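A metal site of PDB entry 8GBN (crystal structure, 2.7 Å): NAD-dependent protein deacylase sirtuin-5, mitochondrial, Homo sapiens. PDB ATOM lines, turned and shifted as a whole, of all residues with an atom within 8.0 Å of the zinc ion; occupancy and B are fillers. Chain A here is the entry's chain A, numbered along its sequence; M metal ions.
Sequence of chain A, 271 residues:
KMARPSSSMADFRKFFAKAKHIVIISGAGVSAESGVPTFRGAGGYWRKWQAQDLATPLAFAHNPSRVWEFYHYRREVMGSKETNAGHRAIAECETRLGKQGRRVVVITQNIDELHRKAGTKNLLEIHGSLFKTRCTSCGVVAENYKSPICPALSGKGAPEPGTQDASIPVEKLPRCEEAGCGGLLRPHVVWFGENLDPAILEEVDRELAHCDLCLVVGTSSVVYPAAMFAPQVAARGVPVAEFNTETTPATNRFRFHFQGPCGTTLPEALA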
ATOM      1  N   ARG A 134     -10.494  -0.121   1.103  1.00  0.00           N
ATOM      2  CA  ARG A 134      -9.641   0.136   2.258  1.00  0.00           C
ATOM      3  C   ARG A 134     -10.084   1.468   2.856  1.00  0.00           C
ATOM      4  O   ARG A 134     -10.246   2.437   2.128  1.00  0.00           O
ATOM      5  CB  ARG A 134      -8.138   0.110   1.896  1.00  0.00           C
ATOM      6  CG  ARG A 134      -7.247   0.195   3.147  1.00  0.00           C
ATOM      7  CD  ARG A 134      -5.818  -0.295   2.932  1.00  0.00           C
ATOM      8  NE  ARG A 134      -4.947   0.705   2.294  1.00  0.00           N
ATOM      9  CZ  ARG A 134      -4.432   0.591   1.077  1.00  0.00           C
ATOM     10  NH1 ARG A 134      -4.673  -0.491   0.346  1.00  0.00           N
ATOM     11  NH2 ARG A 134      -3.659   1.549   0.591  1.00  0.00           N
ATOM     12  N   CYS A 135     -10.359   1.489   4.159  1.00  0.00           N
ATOM     13  CA  CYS A 135     -10.750   2.715   4.820  1.00  0.00           C
ATOM     14  C   CYS A 135      -9.515   3.558   5.049  1.00  0.00           C
ATOM     15  O   CYS A 135      -8.538   3.089   5.634  1.00  0.00           O
ATOM     16  CB  CYS A 135     -11.503   2.444   6.123  1.00  0.00           C
ATOM     17  SG  CYS A 135     -12.142   3.930   6.936  1.00  0.00           S
ATOM     18  N   THR A 136      -9.548   4.812   4.570  1.00  0.00           N
ATOM     19  CA  THR A 136      -8.431   5.739   4.729  1.00  0.00           C
ATOM     20  C   THR A 136      -8.294   6.160   6.203  1.00  0.00           C
ATOM     21  O   THR A 136      -7.269   6.740   6.558  1.00  0.00           O
ATOM     22  CB  THR A 136      -8.619   6.970   3.833  1.00  0.00           C
ATOM     23  OG1 THR A 136      -9.856   7.600   4.160  1.00  0.00           O
ATOM     24  CG2 THR A 136      -8.544   6.647   2.369  1.00  0.00           C
ATOM     25  N   SER A 137      -9.311   5.839   7.037  1.00  0.00           N
ATOM     26  CA  SER A 137      -9.374   6.228   8.430  1.00  0.00           C
ATOM     27  C   SER A 137      -8.977   5.076   9.383  1.00  0.00           C
ATOM     28  O   SER A 137      -8.024   5.243  10.149  1.00  0.00           O
ATOM     29  CB  SER A 137     -10.747   6.811   8.756  1.00  0.00           C
ATOM     30  OG  SER A 137     -11.255   6.407  10.018  1.00  0.00           O
ATOM     31  N   CYS A 138      -9.695   3.917   9.357  1.00  0.00           N
ATOM     32  CA  CYS A 138      -9.413   2.786  10.240  1.00  0.00           C
ATOM     33  C   CYS A 138      -8.524   1.686   9.601  1.00  0.00           C
ATOM     34  O   CYS A 138      -8.097   0.765  10.306  1.00  0.00           O
ATOM     35  CB  CYS A 138     -10.723   2.189  10.751  1.00  0.00           C
ATOM     36  SG  CYS A 138     -11.484   1.016   9.614  1.00  0.00           S
ATOM     37  N   GLY A 139      -8.279   1.772   8.283  1.00  0.00           N
ATOM     38  CA  GLY A 139      -7.458   0.816   7.537  1.00  0.00           C
ATOM     39  C   GLY A 139      -8.051  -0.540   7.210  1.00  0.00           C
ATOM     40  O   GLY A 139      -7.326  -1.386   6.668  1.00  0.00           O
ATOM     41  N   VAL A 140      -9.352  -0.772   7.510  1.00  0.00           N
ATOM     42  CA  VAL A 140      -9.986  -2.074   7.256  1.00  0.00           C
ATOM     43  C   VAL A 140     -10.114  -2.309   5.740  1.00  0.00           C
ATOM     44  O   VAL A 140     -10.419  -1.387   4.994  1.00  0.00           O
ATOM     45  CB  VAL A 140     -11.323  -2.231   8.024  1.00  0.00           C
ATOM     46  CG1 VAL A 140     -12.206  -3.329   7.439  1.00  0.00           C
ATOM     47  CG2 VAL A 140     -11.088  -2.494   9.508  1.00  0.00           C
ATOM     48  N   VAL A 141      -9.832  -3.550   5.324  1.00  0.00           N
ATOM     49  CA  VAL A 141      -9.920  -4.045   3.957  1.00  0.00           C
ATOM     50  C   VAL A 141     -11.188  -4.920   3.870  1.00  0.00           C
ATOM     51  O   VAL A 141     -11.404  -5.793   4.707  1.00  0.00           O
ATOM     52  CB  VAL A 141      -8.617  -4.801   3.535  1.00  0.00           C
ATOM     53  CG1 VAL A 141      -8.691  -5.330   2.080  1.00  0.00           C
ATOM     54  CG2 VAL A 141      -7.410  -3.893   3.724  1.00  0.00           C
ATOM     55  N   ARG A 175     -18.131   5.197   1.927  1.00  0.00           N
ATOM     56  CA  ARG A 175     -17.788   5.344   3.350  1.00  0.00           C
ATOM     57  C   ARG A 175     -17.776   4.009   4.056  1.00  0.00           C
ATOM     58  O   ARG A 175     -18.510   3.105   3.657  1.00  0.00           O
ATOM     59  CB  ARG A 175     -18.755   6.302   4.098  1.00  0.00           C
ATOM     60  CG  ARG A 175     -19.115   7.617   3.396  1.00  0.00           C
ATOM     61  CD  ARG A 175     -17.935   8.526   3.103  1.00  0.00           C
ATOM     62  NE  ARG A 175     -17.300   8.993   4.330  1.00  0.00           N
ATOM     63  CZ  ARG A 175     -16.415   9.982   4.375  1.00  0.00           C
ATOM     64  NH1 ARG A 175     -16.049  10.608   3.265  1.00  0.00           N
ATOM     65  NH2 ARG A 175     -15.872  10.339   5.532  1.00  0.00           N
ATOM     66  N   CYS A 176     -16.958   3.902   5.118  1.00  0.00           N
ATOM     67  CA  CYS A 176     -16.741   2.733   5.967  1.00  0.00           C
ATOM     68  C   CYS A 176     -18.001   2.398   6.776  1.00  0.00           C
ATOM     69  O   CYS A 176     -18.489   3.237   7.542  1.00  0.00           O
ATOM     70  CB  CYS A 176     -15.545   2.978   6.882  1.00  0.00           C
ATOM     71  SG  CYS A 176     -15.043   1.553   7.872  1.00  0.00           S
ATOM     72  N   GLU A 177     -18.506   1.168   6.596  1.00  0.00           N
ATOM     73  CA  GLU A 177     -19.705   0.621   7.245  1.00  0.00           C
ATOM     74  C   GLU A 177     -19.377   0.031   8.640  1.00  0.00           C
ATOM     75  O   GLU A 177     -20.285  -0.513   9.281  1.00  0.00           O
ATOM     76  CB  GLU A 177     -20.374  -0.433   6.348  1.00  0.00           C
ATOM     77  CG  GLU A 177     -21.216   0.162   5.225  1.00  0.00           C
ATOM     78  CD  GLU A 177     -21.196  -0.557   3.892  1.00  0.00           C
ATOM     79  OE1 GLU A 177     -21.172   0.150   2.855  1.00  0.00           O
ATOM     80  OE2 GLU A 177     -21.216  -1.810   3.864  1.00  0.00           O
ATOM     81  N   GLU A 178     -18.114   0.165   9.112  1.00  0.00           N
ATOM     82  CA  GLU A 178     -17.712  -0.235  10.469  1.00  0.00           C
ATOM     83  C   GLU A 178     -18.339   0.720  11.464  1.00  0.00           C
ATOM     84  O   GLU A 178     -18.429   1.934  11.195  1.00  0.00           O
ATOM     85  CB  GLU A 178     -16.175  -0.271  10.660  1.00  0.00           C
ATOM     86  CG  GLU A 178     -15.454  -1.362   9.881  1.00  0.00           C
ATOM     87  CD  GLU A 178     -15.286  -2.670  10.623  1.00  0.00           C
ATOM     88  OE1 GLU A 178     -14.137  -2.976  11.045  1.00  0.00           O
ATOM     89  OE2 GLU A 178     -16.286  -3.402  10.786  1.00  0.00           O
ATOM     90  N   ALA A 179     -18.823   0.178  12.592  1.00  0.00           N
ATOM     91  CA  ALA A 179     -19.512   0.949  13.613  1.00  0.00           C
ATOM     92  C   ALA A 179     -18.630   2.055  14.193  1.00  0.00           C
ATOM     93  O   ALA A 179     -17.573   1.787  14.787  1.00  0.00           O
ATOM     94  CB  ALA A 179     -20.014   0.025  14.705  1.00  0.00           C
ATOM     95  N   GLY A 180     -19.069   3.292  13.990  1.00  0.00           N
ATOM     96  CA  GLY A 180     -18.418   4.487  14.492  1.00  0.00           C
ATOM     97  C   GLY A 180     -17.170   4.924  13.742  1.00  0.00           C
ATOM     98  O   GLY A 180     -16.295   5.579  14.307  1.00  0.00           O
ATOM     99  N   CYS A 181     -17.069   4.542  12.451  1.00  0.00           N
ATOM    100  CA  CYS A 181     -15.944   4.954  11.655  1.00  0.00           C
ATOM    101  C   CYS A 181     -16.400   6.016  10.650  1.00  0.00           C
ATOM    102  O   CYS A 181     -16.089   7.192  10.805  1.00  0.00           O
ATOM    103  CB  CYS A 181     -15.256   3.775  10.976  1.00  0.00           C
ATOM    104  SG  CYS A 181     -13.793   4.223  10.010  1.00  0.00           S
ATOM    105  N   GLY A 182     -17.140   5.576   9.621  1.00  0.00           N
ATOM    106  CA  GLY A 182     -17.647   6.442   8.568  1.00  0.00           C
ATOM    107  C   GLY A 182     -16.595   7.115   7.708  1.00  0.00           C
ATOM    108  O   GLY A 182     -16.909   8.033   6.960  1.00  0.00           O
ATOM    109  N   GLY A 183     -15.355   6.647   7.817  1.00  0.00           N
ATOM    110  CA  GLY A 183     -14.219   7.166   7.063  1.00  0.00           C
ATOM    111  C   GLY A 183     -14.339   6.945   5.581  1.00  0.00           C
ATOM    112  O   GLY A 183     -15.050   6.046   5.128  1.00  0.00           O
ATOM    113  N   LEU A 184     -13.653   7.803   4.809  1.00  0.00           N
ATOM    114  CA  LEU A 184     -13.642   7.778   3.364  1.00  0.00           C
ATOM    115  C   LEU A 184     -12.925   6.512   2.851  1.00  0.00           C
ATOM    116  O   LEU A 184     -11.780   6.257   3.204  1.00  0.00           O
ATOM    117  CB  LEU A 184     -12.992   9.074   2.796  1.00  0.00           C
ATOM    118  CG  LEU A 184     -12.872   9.232   1.272  1.00  0.00           C
ATOM    119  CD1 LEU A 184     -14.231   9.173   0.569  1.00  0.00           C
ATOM    120  CD2 LEU A 184     -12.093  10.472   0.914  1.00  0.00           C
ATOM    121  N   LEU A 185     -13.644   5.691   2.070  1.00  0.00           N
ATOM    122  CA  LEU A 185     -13.043   4.500   1.492  1.00  0.00           C
ATOM    123  C   LEU A 185     -12.266   4.847   0.233  1.00  0.00           C
ATOM    124  O   LEU A 185     -12.574   5.820  -0.456  1.00  0.00           O
ATOM    125  CB  LEU A 185     -14.101   3.435   1.154  1.00  0.00           C
ATOM    126  CG  LEU A 185     -14.822   2.744   2.278  1.00  0.00           C
ATOM    127  CD1 LEU A 185     -15.882   1.822   1.703  1.00  0.00           C
ATOM    128  CD2 LEU A 185     -13.865   1.946   3.148  1.00  0.00           C
HETATM  129 ZN    ZN M   1     -13.098   2.572   8.665  1.00  0.00          ZN
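Four residues have an atom within 4 Å of the zinc ion: Cys 135, Cys 138, Cys 176 and Cys 181.
The zinc ion is bound by the side-chain sulfur (SG) of Cys 181 (2.2 Å), the side-chain sulfur (SG) of Cys 176 (2.3 Å), the side-chain sulfur (SG) of Cys 135 (2.4 Å) and the side-chain sulfur (SG) of Cys 138 (2.4 Å).
OG of Ser 137 sits close to SG of Cys 181 (3.3 Å). The backbone NH (N) of Gly 183 lies close to the side-chain sulfur (SG) of Cys 181. The side-chain sulfur (SG) of Cys 176 sits close to the backbone NH (N) of Glu 178 (3.6 Å). The backbone carbonyl oxygen (O) of Gly 183 is in hydrogen-bond range of the backbone NH (N) of Cys 176, at 2.9 Å. The backbone NH (N) of Gly 182 is in hydrogen-bond range of the backbone carbonyl oxygen (O) of Cys 176, at 3.4 Å. The backbone NH of Ser 137 sits close to the side-chain sulfur of Cys 135 (3.4 Å). The backbone NH of Cys 135 is in hydrogen-bond range of the backbone carbonyl oxygen of Val 140 (3.0 Å). The backbone NH (N) of Val 140 lies close to the side-chain sulfur (SG) of Cys 138, at 3.5 Å.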
